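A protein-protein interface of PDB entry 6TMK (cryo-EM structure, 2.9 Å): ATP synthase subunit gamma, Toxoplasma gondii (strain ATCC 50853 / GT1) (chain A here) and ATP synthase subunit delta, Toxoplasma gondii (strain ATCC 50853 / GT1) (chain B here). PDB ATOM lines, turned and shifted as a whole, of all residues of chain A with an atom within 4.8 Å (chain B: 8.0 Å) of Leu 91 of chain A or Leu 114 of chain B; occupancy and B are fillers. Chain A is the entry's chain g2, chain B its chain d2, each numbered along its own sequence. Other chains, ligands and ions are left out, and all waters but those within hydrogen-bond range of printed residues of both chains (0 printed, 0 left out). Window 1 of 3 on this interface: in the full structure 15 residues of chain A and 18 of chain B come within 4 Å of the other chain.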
ATOM      1  N   PRO A  87     -18.719 -26.373  22.562  1.00  0.00           N
ATOM      2  CA  PRO A  87     -19.920 -25.620  22.172  1.00  0.00           C
ATOM      3  C   PRO A  87     -21.078 -25.926  23.099  1.00  0.00           C
ATOM      4  O   PRO A  87     -21.747 -25.011  23.601  1.00  0.00           O
ATOM      5  CB  PRO A  87     -20.175 -26.095  20.734  1.00  0.00           C
ATOM      6  CG  PRO A  87     -18.855 -26.614  20.262  1.00  0.00           C
ATOM      7  CD  PRO A  87     -18.230 -27.229  21.471  1.00  0.00           C
ATOM      8  N   VAL A  88     -21.329 -27.215  23.346  1.00  0.00           N
ATOM      9  CA  VAL A  88     -22.450 -27.606  24.188  1.00  0.00           C
ATOM     10  C   VAL A  88     -22.207 -27.179  25.629  1.00  0.00           C
ATOM     11  O   VAL A  88     -23.151 -26.803  26.344  1.00  0.00           O
ATOM     12  CB  VAL A  88     -22.700 -29.121  24.074  1.00  0.00           C
ATOM     13  CG1 VAL A  88     -21.617 -29.899  24.794  1.00  0.00           C
ATOM     14  CG2 VAL A  88     -24.069 -29.469  24.625  1.00  0.00           C
ATOM     15  N   GLN A  89     -20.945 -27.204  26.081  1.00  0.00           N
ATOM     16  CA  GLN A  89     -20.678 -26.735  27.436  1.00  0.00           C
ATOM     17  C   GLN A  89     -20.975 -25.248  27.577  1.00  0.00           C
ATOM     18  O   GLN A  89     -21.585 -24.832  28.563  1.00  0.00           O
ATOM     19  CB  GLN A  89     -19.234 -27.031  27.833  1.00  0.00           C
ATOM     20  CG  GLN A  89     -18.903 -28.507  27.926  1.00  0.00           C
ATOM     21  CD  GLN A  89     -17.447 -28.754  28.253  1.00  0.00           C
ATOM     22  OE1 GLN A  89     -16.635 -29.020  27.369  1.00  0.00           O
ATOM     23  NE2 GLN A  89     -17.110 -28.666  29.533  1.00  0.00           N
ATOM     24  N   LYS A  90     -20.557 -24.435  26.606  1.00  0.00           N
ATOM     25  CA  LYS A  90     -20.867 -23.007  26.650  1.00  0.00           C
ATOM     26  C   LYS A  90     -22.364 -22.755  26.547  1.00  0.00           C
ATOM     27  O   LYS A  90     -22.907 -21.875  27.235  1.00  0.00           O
ATOM     28  CB  LYS A  90     -20.135 -22.289  25.518  1.00  0.00           C
ATOM     29  CG  LYS A  90     -18.677 -22.001  25.812  1.00  0.00           C
ATOM     30  CD  LYS A  90     -17.986 -21.383  24.611  1.00  0.00           C
ATOM     31  CE  LYS A  90     -16.529 -21.073  24.907  1.00  0.00           C
ATOM     32  NZ  LYS A  90     -15.742 -20.852  23.666  1.00  0.00           N
ATOM     33  N   LEU A  91     -23.062 -23.592  25.779  1.00  0.00           N
ATOM     34  CA  LEU A  91     -24.507 -23.454  25.676  1.00  0.00           C
ATOM     35  C   LEU A  91     -25.156 -23.661  27.031  1.00  0.00           C
ATOM     36  O   LEU A  91     -25.933 -22.817  27.493  1.00  0.00           O
ATOM     37  CB  LEU A  91     -25.057 -24.444  24.650  1.00  0.00           C
ATOM     38  CG  LEU A  91     -26.575 -24.449  24.473  1.00  0.00           C
ATOM     39  CD1 LEU A  91     -27.059 -23.111  23.951  1.00  0.00           C
ATOM     40  CD2 LEU A  91     -26.983 -25.559  23.533  1.00  0.00           C
ATOM     41  N   VAL A  92     -24.855 -24.778  27.693  1.00  0.00           N
ATOM     42  CA  VAL A  92     -25.566 -25.015  28.941  1.00  0.00           C
ATOM     43  C   VAL A  92     -25.032 -24.090  30.027  1.00  0.00           C
ATOM     44  O   VAL A  92     -25.745 -23.774  30.986  1.00  0.00           O
ATOM     45  CB  VAL A  92     -25.452 -26.491  29.356  1.00  0.00           C
ATOM     46  CG1 VAL A  92     -26.166 -26.723  30.675  1.00  0.00           C
ATOM     47  CG2 VAL A  92     -26.022 -27.387  28.274  1.00  0.00           C
ATOM     48  N   GLN A  93     -23.780 -23.638  29.902  1.00  0.00           N
ATOM     49  CA  GLN A  93     -23.212 -22.690  30.848  1.00  0.00           C
ATOM     50  C   GLN A  93     -23.834 -21.310  30.727  1.00  0.00           C
ATOM     51  O   GLN A  93     -23.658 -20.489  31.632  1.00  0.00           O
ATOM     52  CB  GLN A  93     -21.700 -22.597  30.646  1.00  0.00           C
ATOM     53  CG  GLN A  93     -20.929 -23.758  31.250  1.00  0.00           C
ATOM     54  CD  GLN A  93     -19.526 -23.879  30.694  1.00  0.00           C
ATOM     55  OE1 GLN A  93     -19.011 -22.952  30.069  1.00  0.00           O
ATOM     56  NE2 GLN A  93     -18.898 -25.027  30.919  1.00  0.00           N
ATOM     57  N   ARG A  94     -24.551 -21.036  29.635  1.00  0.00           N
ATOM     58  CA  ARG A  94     -25.317 -19.794  29.582  1.00  0.00           C
ATOM     59  C   ARG A  94     -26.309 -19.712  30.735  1.00  0.00           C
ATOM     60  O   ARG A  94     -26.626 -18.614  31.208  1.00  0.00           O
ATOM     61  CB  ARG A  94     -26.053 -19.674  28.250  1.00  0.00           C
ATOM     62  CG  ARG A  94     -25.158 -19.359  27.071  1.00  0.00           C
ATOM     63  CD  ARG A  94     -25.906 -19.516  25.762  1.00  0.00           C
ATOM     64  NE  ARG A  94     -27.022 -18.575  25.663  1.00  0.00           N
ATOM     65  CZ  ARG A  94     -27.261 -17.780  24.623  1.00  0.00           C
ATOM     66  NH1 ARG A  94     -26.475 -17.791  23.555  1.00  0.00           N
ATOM     67  NH2 ARG A  94     -28.305 -16.967  24.648  1.00  0.00           N
ATOM     68  N   ILE A  95     -26.807 -20.854  31.195  1.00  0.00           N
ATOM     69  CA  ILE A  95     -27.657 -20.939  32.380  1.00  0.00           C
ATOM     70  C   ILE A  95     -26.779 -20.862  33.624  1.00  0.00           C
ATOM     71  O   ILE A  95     -26.116 -21.852  33.968  1.00  0.00           O
ATOM     72  CB  ILE A  95     -28.497 -22.224  32.378  1.00  0.00           C
ATOM     73  CG1 ILE A  95     -29.457 -22.229  31.189  1.00  0.00           C
ATOM     74  CG2 ILE A  95     -29.272 -22.352  33.679  1.00  0.00           C
ATOM     75  CD1 ILE A  95     -29.972 -23.600  30.842  1.00  0.00           C
ATOM     76  N   LEU A 229     -32.431 -19.443  26.633  1.00  0.00           N
ATOM     77  CA  LEU A 229     -32.323 -20.204  25.396  1.00  0.00           C
ATOM     78  C   LEU A 229     -33.476 -19.935  24.440  1.00  0.00           C
ATOM     79  O   LEU A 229     -33.595 -20.625  23.422  1.00  0.00           O
ATOM     80  CB  LEU A 229     -32.252 -21.698  25.707  1.00  0.00           C
ATOM     81  CG  LEU A 229     -31.279 -22.100  26.812  1.00  0.00           C
ATOM     82  CD1 LEU A 229     -31.310 -23.602  27.023  1.00  0.00           C
ATOM     83  CD2 LEU A 229     -29.879 -21.630  26.475  1.00  0.00           C
ATOM     84  N   PHE A 232     -32.857 -19.539  20.778  1.00  0.00           N
ATOM     85  CA  PHE A 232     -32.510 -20.718  20.000  1.00  0.00           C
ATOM     86  C   PHE A 232     -33.766 -21.478  19.595  1.00  0.00           C
ATOM     87  O   PHE A 232     -34.713 -21.600  20.377  1.00  0.00           O
ATOM     88  CB  PHE A 232     -31.591 -21.643  20.799  1.00  0.00           C
ATOM     89  CG  PHE A 232     -30.141 -21.275  20.716  1.00  0.00           C
ATOM     90  CD1 PHE A 232     -29.606 -20.324  21.565  1.00  0.00           C
ATOM     91  CD2 PHE A 232     -29.314 -21.877  19.785  1.00  0.00           C
ATOM     92  CE1 PHE A 232     -28.273 -19.985  21.491  1.00  0.00           C
ATOM     93  CE2 PHE A 232     -27.981 -21.541  19.706  1.00  0.00           C
ATOM     94  CZ  PHE A 232     -27.459 -20.594  20.560  1.00  0.00           C
ATOM     95  N   LEU A 245     -30.205 -33.369  25.655  1.00  0.00           N
ATOM     96  CA  LEU A 245     -29.129 -32.403  25.561  1.00  0.00           C
ATOM     97  C   LEU A 245     -28.384 -32.393  26.881  1.00  0.00           C
ATOM     98  O   LEU A 245     -27.166 -32.195  26.906  1.00  0.00           O
ATOM     99  CB  LEU A 245     -29.682 -31.023  25.224  1.00  0.00           C
ATOM    100  CG  LEU A 245     -28.668 -29.887  25.143  1.00  0.00           C
ATOM    101  CD1 LEU A 245     -27.677 -30.139  24.026  1.00  0.00           C
ATOM    102  CD2 LEU A 245     -29.388 -28.575  24.932  1.00  0.00           C
ATOM    103  N   LEU B  45     -20.045 -19.364   5.932  1.00  0.00           N
ATOM    104  CA  LEU B  45     -20.520 -20.279   6.959  1.00  0.00           C
ATOM    105  C   LEU B  45     -19.324 -21.066   7.482  1.00  0.00           C
ATOM    106  O   LEU B  45     -18.716 -21.850   6.746  1.00  0.00           O
ATOM    107  CB  LEU B  45     -21.589 -21.212   6.397  1.00  0.00           C
ATOM    108  CG  LEU B  45     -22.189 -22.250   7.348  1.00  0.00           C
ATOM    109  CD1 LEU B  45     -22.867 -21.584   8.529  1.00  0.00           C
ATOM    110  CD2 LEU B  45     -23.166 -23.144   6.612  1.00  0.00           C
ATOM    111  N   LEU B  46     -19.002 -20.849   8.750  1.00  0.00           N
ATOM    112  CA  LEU B  46     -17.868 -21.472   9.425  1.00  0.00           C
ATOM    113  C   LEU B  46     -18.349 -22.795  10.000  1.00  0.00           C
ATOM    114  O   LEU B  46     -18.937 -22.834  11.083  1.00  0.00           O
ATOM    115  CB  LEU B  46     -17.325 -20.552  10.509  1.00  0.00           C
ATOM    116  CG  LEU B  46     -16.460 -19.400   9.998  1.00  0.00           C
ATOM    117  CD1 LEU B  46     -16.538 -18.211  10.942  1.00  0.00           C
ATOM    118  CD2 LEU B  46     -15.029 -19.850   9.817  1.00  0.00           C
ATOM    119  N   LEU B  47     -18.105 -23.886   9.283  1.00  0.00           N
ATOM    120  CA  LEU B  47     -18.473 -25.204   9.771  1.00  0.00           C
ATOM    121  C   LEU B  47     -17.363 -25.771  10.641  1.00  0.00           C
ATOM    122  O   LEU B  47     -16.176 -25.604  10.345  1.00  0.00           O
ATOM    123  CB  LEU B  47     -18.745 -26.154   8.604  1.00  0.00           C
ATOM    124  CG  LEU B  47     -19.241 -27.547   8.988  1.00  0.00           C
ATOM    125  CD1 LEU B  47     -20.701 -27.503   9.403  1.00  0.00           C
ATOM    126  CD2 LEU B  47     -19.030 -28.516   7.840  1.00  0.00           C
ATOM    127  N   THR B  48     -17.759 -26.443  11.720  1.00  0.00           N
ATOM    128  CA  THR B  48     -16.892 -27.384  12.419  1.00  0.00           C
ATOM    129  C   THR B  48     -17.643 -28.698  12.593  1.00  0.00           C
ATOM    130  O   THR B  48     -18.652 -28.754  13.303  1.00  0.00           O
ATOM    131  CB  THR B  48     -16.427 -26.825  13.767  1.00  0.00           C
ATOM    132  OG1 THR B  48     -15.542 -27.763  14.395  1.00  0.00           O
ATOM    133  CG2 THR B  48     -17.599 -26.548  14.692  1.00  0.00           C
ATOM    134  N   MET B  76     -28.388 -26.139   6.278  1.00  0.00           N
ATOM    135  CA  MET B  76     -28.054 -24.880   6.923  1.00  0.00           C
ATOM    136  C   MET B  76     -27.150 -24.058   6.017  1.00  0.00           C
ATOM    137  O   MET B  76     -26.207 -24.583   5.418  1.00  0.00           O
ATOM    138  CB  MET B  76     -27.372 -25.117   8.271  1.00  0.00           C
ATOM    139  CG  MET B  76     -28.286 -25.716   9.321  1.00  0.00           C
ATOM    140  SD  MET B  76     -27.453 -26.029  10.888  1.00  0.00           S
ATOM    141  CE  MET B  76     -28.801 -26.714  11.848  1.00  0.00           C
ATOM    142  N   SER B  81     -31.377 -19.133  11.009  1.00  0.00           N
ATOM    143  CA  SER B  81     -31.652 -18.710  12.371  1.00  0.00           C
ATOM    144  C   SER B  81     -30.849 -19.545  13.366  1.00  0.00           C
ATOM    145  O   SER B  81     -30.423 -20.668  13.078  1.00  0.00           O
ATOM    146  CB  SER B  81     -33.144 -18.826  12.677  1.00  0.00           C
ATOM    147  OG  SER B  81     -33.395 -18.632  14.057  1.00  0.00           O
ATOM    148  N   GLN B  82     -30.640 -18.979  14.550  1.00  0.00           N
ATOM    149  CA  GLN B  82     -30.091 -19.752  15.654  1.00  0.00           C
ATOM    150  C   GLN B  82     -30.999 -20.940  15.936  1.00  0.00           C
ATOM    151  O   GLN B  82     -32.197 -20.769  16.179  1.00  0.00           O
ATOM    152  CB  GLN B  82     -29.952 -18.889  16.906  1.00  0.00           C
ATOM    153  CG  GLN B  82     -28.939 -17.774  16.797  1.00  0.00           C
ATOM    154  CD  GLN B  82     -28.854 -16.954  18.068  1.00  0.00           C
ATOM    155  OE1 GLN B  82     -29.564 -17.217  19.039  1.00  0.00           O
ATOM    156  NE2 GLN B  82     -27.978 -15.957  18.072  1.00  0.00           N
ATOM    157  N   THR B  83     -30.436 -22.146  15.906  1.00  0.00           N
ATOM    158  CA  THR B  83     -31.244 -23.332  16.132  1.00  0.00           C
ATOM    159  C   THR B  83     -30.385 -24.445  16.705  1.00  0.00           C
ATOM    160  O   THR B  83     -29.162 -24.469  16.543  1.00  0.00           O
ATOM    161  CB  THR B  83     -31.915 -23.811  14.837  1.00  0.00           C
ATOM    162  OG1 THR B  83     -32.810 -24.891  15.129  1.00  0.00           O
ATOM    163  CG2 THR B  83     -30.873 -24.283  13.833  1.00  0.00           C
ATOM    164  N   VAL B  84     -31.058 -25.369  17.382  1.00  0.00           N
ATOM    165  CA  VAL B  84     -30.470 -26.608  17.869  1.00  0.00           C
ATOM    166  C   VAL B  84     -31.341 -27.753  17.380  1.00  0.00           C
ATOM    167  O   VAL B  84     -32.568 -27.628  17.323  1.00  0.00           O
ATOM    168  CB  VAL B  84     -30.364 -26.625  19.407  1.00  0.00           C
ATOM    169  CG1 VAL B  84     -29.741 -27.921  19.880  1.00  0.00           C
ATOM    170  CG2 VAL B  84     -29.571 -25.431  19.890  1.00  0.00           C
ATOM    171  N   ALA B  85     -30.710 -28.866  17.020  1.00  0.00           N
ATOM    172  CA  ALA B  85     -31.454 -30.005  16.514  1.00  0.00           C
ATOM    173  C   ALA B  85     -30.721 -31.287  16.865  1.00  0.00           C
ATOM    174  O   ALA B  85     -29.493 -31.319  16.961  1.00  0.00           O
ATOM    175  CB  ALA B  85     -31.664 -29.913  14.999  1.00  0.00           C
ATOM    176  N   ARG B  86     -31.502 -32.342  17.059  1.00  0.00           N
ATOM    177  CA  ARG B  86     -30.994 -33.678  17.318  1.00  0.00           C
ATOM    178  C   ARG B  86     -30.988 -34.465  16.017  1.00  0.00           C
ATOM    179  O   ARG B  86     -31.922 -34.362  15.217  1.00  0.00           O
ATOM    180  CB  ARG B  86     -31.867 -34.374  18.360  1.00  0.00           C
ATOM    181  CG  ARG B  86     -31.432 -35.762  18.763  1.00  0.00           C
ATOM    182  CD  ARG B  86     -32.362 -36.278  19.834  1.00  0.00           C
ATOM    183  NE  ARG B  86     -33.543 -36.910  19.254  1.00  0.00           N
ATOM    184  CZ  ARG B  86     -34.708 -37.046  19.882  1.00  0.00           C
ATOM    185  NH1 ARG B  86     -34.860 -36.598  21.121  1.00  0.00           N
ATOM    186  NH2 ARG B  86     -35.723 -37.637  19.268  1.00  0.00           N
ATOM    187  N   LEU B  87     -29.940 -35.253  15.810  1.00  0.00           N
ATOM    188  CA  LEU B  87     -29.807 -36.054  14.606  1.00  0.00           C
ATOM    189  C   LEU B  87     -29.998 -37.531  14.918  1.00  0.00           C
ATOM    190  O   LEU B  87     -29.793 -37.986  16.047  1.00  0.00           O
ATOM    191  CB  LEU B  87     -28.433 -35.843  13.964  1.00  0.00           C
ATOM    192  CG  LEU B  87     -27.906 -34.408  13.938  1.00  0.00           C
ATOM    193  CD1 LEU B  87     -26.549 -34.363  13.264  1.00  0.00           C
ATOM    194  CD2 LEU B  87     -28.875 -33.475  13.248  1.00  0.00           C
ATOM    195  N   PHE B 112     -25.736 -33.936  17.780  1.00  0.00           N
ATOM    196  CA  PHE B 112     -26.425 -32.661  17.871  1.00  0.00           C
ATOM    197  C   PHE B 112     -25.829 -31.703  16.852  1.00  0.00           C
ATOM    198  O   PHE B 112     -24.737 -31.923  16.323  1.00  0.00           O
ATOM    199  CB  PHE B 112     -26.331 -32.062  19.278  1.00  0.00           C
ATOM    200  CG  PHE B 112     -27.347 -32.602  20.232  1.00  0.00           C
ATOM    201  CD1 PHE B 112     -27.142 -33.808  20.872  1.00  0.00           C
ATOM    202  CD2 PHE B 112     -28.513 -31.905  20.487  1.00  0.00           C
ATOM    203  CE1 PHE B 112     -28.079 -34.309  21.750  1.00  0.00           C
ATOM    204  CE2 PHE B 112     -29.454 -32.398  21.365  1.00  0.00           C
ATOM    205  CZ  PHE B 112     -29.238 -33.602  21.996  1.00  0.00           C
ATOM    206  N   VAL B 113     -26.568 -30.632  16.582  1.00  0.00           N
ATOM    207  CA  VAL B 113     -26.112 -29.554  15.715  1.00  0.00           C
ATOM    208  C   VAL B 113     -26.449 -28.230  16.380  1.00  0.00           C
ATOM    209  O   VAL B 113     -27.519 -28.076  16.976  1.00  0.00           O
ATOM    210  CB  VAL B 113     -26.747 -29.641  14.314  1.00  0.00           C
ATOM    211  CG1 VAL B 113     -28.226 -29.366  14.391  1.00  0.00           C
ATOM    212  CG2 VAL B 113     -26.085 -28.655  13.379  1.00  0.00           C
ATOM    213  N   LEU B 114     -25.529 -27.274  16.276  1.00  0.00           N
ATOM    214  CA  LEU B 114     -25.656 -25.978  16.931  1.00  0.00           C
ATOM    215  C   LEU B 114     -25.301 -24.895  15.924  1.00  0.00           C
ATOM    216  O   LEU B 114     -24.134 -24.750  15.550  1.00  0.00           O
ATOM    217  CB  LEU B 114     -24.748 -25.890  18.157  1.00  0.00           C
ATOM    218  CG  LEU B 114     -24.980 -26.924  19.258  1.00  0.00           C
ATOM    219  CD1 LEU B 114     -23.749 -27.032  20.136  1.00  0.00           C
ATOM    220  CD2 LEU B 114     -26.193 -26.567  20.093  1.00  0.00           C
ATOM    221  N   PHE B 115     -26.306 -24.145  15.486  1.00  0.00           N
ATOM    222  CA  PHE B 115     -26.122 -23.053  14.542  1.00  0.00           C
ATOM    223  C   PHE B 115     -26.221 -21.742  15.311  1.00  0.00           C
ATOM    224  O   PHE B 115     -27.256 -21.454  15.923  1.00  0.00           O
ATOM    225  CB  PHE B 115     -27.164 -23.108  13.428  1.00  0.00           C
ATOM    226  CG  PHE B 115     -26.828 -22.251  12.247  1.00  0.00           C
ATOM    227  CD1 PHE B 115     -26.227 -22.798  11.128  1.00  0.00           C
ATOM    228  CD2 PHE B 115     -27.113 -20.900  12.256  1.00  0.00           C
ATOM    229  CE1 PHE B 115     -25.918 -22.012  10.040  1.00  0.00           C
ATOM    230  CE2 PHE B 115     -26.804 -20.109  11.171  1.00  0.00           C
ATOM    231  CZ  PHE B 115     -26.205 -20.665  10.062  1.00  0.00           C
ATOM    232  N   LYS B 116     -25.149 -20.956  15.283  1.00  0.00           N
ATOM    233  CA  LYS B 116     -25.060 -19.717  16.040  1.00  0.00           C
ATOM    234  C   LYS B 116     -24.927 -18.540  15.088  1.00  0.00           C
ATOM    235  O   LYS B 116     -24.134 -18.585  14.142  1.00  0.00           O
ATOM    236  CB  LYS B 116     -23.870 -19.745  17.004  1.00  0.00           C
ATOM    237  CG  LYS B 116     -24.173 -20.399  18.340  1.00  0.00           C
ATOM    238  CD  LYS B 116     -22.991 -20.305  19.287  1.00  0.00           C
ATOM    239  CE  LYS B 116     -21.879 -21.258  18.881  1.00  0.00           C
ATOM    240  NZ  LYS B 116     -20.852 -21.410  19.948  1.00  0.00           N
ATOM    241  N   SER B 117     -25.707 -17.492  15.345  1.00  0.00           N
ATOM    242  CA  SER B 117     -25.735 -16.341  14.465  1.00  0.00           C
ATOM    243  C   SER B 117     -24.355 -15.692  14.434  1.00  0.00           C
ATOM    244  O   SER B 117     -23.519 -15.944  15.305  1.00  0.00           O
ATOM    245  CB  SER B 117     -26.785 -15.337  14.937  1.00  0.00           C
ATOM    246  OG  SER B 117     -26.319 -14.600  16.053  1.00  0.00           O
ATOM    247  N   THR B 126     -21.559 -19.192  12.109  1.00  0.00           N
ATOM    248  CA  THR B 126     -20.880 -20.422  12.490  1.00  0.00           C
ATOM    249  C   THR B 126     -21.873 -21.547  12.758  1.00  0.00           C
ATOM    250  O   THR B 126     -23.047 -21.320  13.063  1.00  0.00           O
ATOM    251  CB  THR B 126     -20.007 -20.200  13.732  1.00  0.00           C
ATOM    252  OG1 THR B 126     -19.103 -21.301  13.889  1.00  0.00           O
ATOM    253  CG2 THR B 126     -20.868 -20.069  14.979  1.00  0.00           C
ATOM    254  N   ALA B 127     -21.371 -22.777  12.642  1.00  0.00           N
ATOM    255  CA  ALA B 127     -22.180 -23.977  12.777  1.00  0.00           C
ATOM    256  C   ALA B 127     -21.302 -25.103  13.301  1.00  0.00           C
ATOM    257  O   ALA B 127     -20.135 -25.222  12.915  1.00  0.00           O
ATOM    258  CB  ALA B 127     -22.812 -24.381  11.442  1.00  0.00           C
ATOM    259  N   GLU B 128     -21.876 -25.932  14.172  1.00  0.00           N
ATOM    260  CA  GLU B 128     -21.147 -26.993  14.857  1.00  0.00           C
ATOM    261  C   GLU B 128     -21.946 -28.283  14.771  1.00  0.00           C
ATOM    262  O   GLU B 128     -23.062 -28.360  15.297  1.00  0.00           O
ATOM    263  CB  GLU B 128     -20.887 -26.626  16.319  1.00  0.00           C
ATOM    264  CG  GLU B 128     -20.036 -25.383  16.498  1.00  0.00           C
ATOM    265  CD  GLU B 128     -20.785 -24.251  17.173  1.00  0.00           C
ATOM    266  OE1 GLU B 128     -21.960 -24.021  16.823  1.00  0.00           O
ATOM    267  OE2 GLU B 128     -20.195 -23.589  18.052  1.00  0.00           O
ATOM    268  N   VAL B 129     -21.377 -29.287  14.114  1.00  0.00           N
ATOM    269  CA  VAL B 129     -22.019 -30.578  13.908  1.00  0.00           C
ATOM    270  C   VAL B 129     -21.238 -31.612  14.708  1.00  0.00           C
ATOM    271  O   VAL B 129     -20.133 -32.013  14.318  1.00  0.00           O
ATOM    272  CB  VAL B 129     -22.080 -30.955  12.423  1.00  0.00           C
ATOM    273  CG1 VAL B 129     -22.750 -32.300  12.250  1.00  0.00           C
ATOM    274  CG2 VAL B 129     -22.823 -29.892  11.642  1.00  0.00           C
ATOM    275  N   LEU B 130     -21.821 -32.057  15.818  1.00  0.00           N
ATOM    276  CA  LEU B 130     -21.170 -32.978  16.737  1.00  0.00           C
ATOM    277  C   LEU B 130     -21.743 -34.374  16.550  1.00  0.00           C
ATOM    278  O   LEU B 130     -22.963 -34.563  16.588  1.00  0.00           O
ATOM    279  CB  LEU B 130     -21.357 -32.527  18.185  1.00  0.00           C
ATOM    280  CG  LEU B 130     -21.244 -31.024  18.435  1.00  0.00           C
ATOM    281  CD1 LEU B 130     -21.576 -30.701  19.879  1.00  0.00           C
ATOM    282  CD2 LEU B 130     -19.856 -30.536  18.074  1.00  0.00           C
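OG of Ser 117 of chain B is in hydrogen-bond range of NE2 of Gln 82 of chain B, at 2.9 Å. O of Thr 83 of chain B lies within hydrogen-bond range of N of Phe 115 of chain B (3.1 Å). The backbone carbonyl oxygen (O) of Phe 112 of chain B sits at hydrogen-bond distance from the backbone NH (N) of Leu 130 of chain B (3.0 Å). N of Leu 114 of chain B is in hydrogen-bond range of O of Glu 128 of chain B, 2.9 Å away. The backbone NH (N) of Lys 116 of chain B sits at hydrogen-bond distance from the backbone carbonyl oxygen (O) of Thr 126 of chain B (3.1 Å). The side-chain amino group (NZ) of Lys 116 of chain B is in salt-bridge range of the side-chain carboxylate (OE2) of Glu 128 of chain B.
Among the printed residues, merely in contact across the chains: Phe 232 of chain A with Val 84 of chain B, Pro 87 of chain A with Glu 128 of chain B, Leu 91 of chain A with Leu 114 of chain B, Pro 87 of chain A with Leu 114 of chain B, Leu 245 of chain A with Phe 112 of chain B, Phe 232 of chain A with Gln 82 of chain B, Phe 232 of chain A with Phe 115 of chain B and Phe 232 of chain A with Lys 116 of chain B.
Leu 91 of chain A touches just one residue of chain B: Leu 114. Of chain A, only Pro 87 and Leu 91 come within 4 Å of Leu 114 of chain B. Of the printed residues of chain A, Phe 115 of chain B touches Phe 232 (3.9 Å). Of the printed residues of chain A, Phe 112 of chain B touches Leu 245 (3.8 Å). Of the printed residues of chain A, Val 84 of chain B touches Phe 232 (3.6 Å). Arg 94 of chain A touches none of the printed residues of chain B. Gln 93 of chain A touches none of the printed residues of chain B. The nearest residue of chain B that does not touch Leu 91 of chain A is Val 84 of chain B (4.5 Å). The nearest residue of chain A that does not touch Leu 114 of chain B is Val 88 of chain A (4.02 Å).
Hydrophobic or aromatic side chains of chain A within 4 Å of the printed part of chain B: Pro 87, Leu 91, Phe 232 and Leu 245. Hydrophobic or aromatic side chains of chain B that line the printed part of chain A: Val 84, Phe 112 and Leu 114. Among the printed residues, 8 pairs touch across the chains. Among the printed residues, no Asp or Glu carboxylate lies within 4 Å of a Lys or Arg side-chain nitrogen of the other chain.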
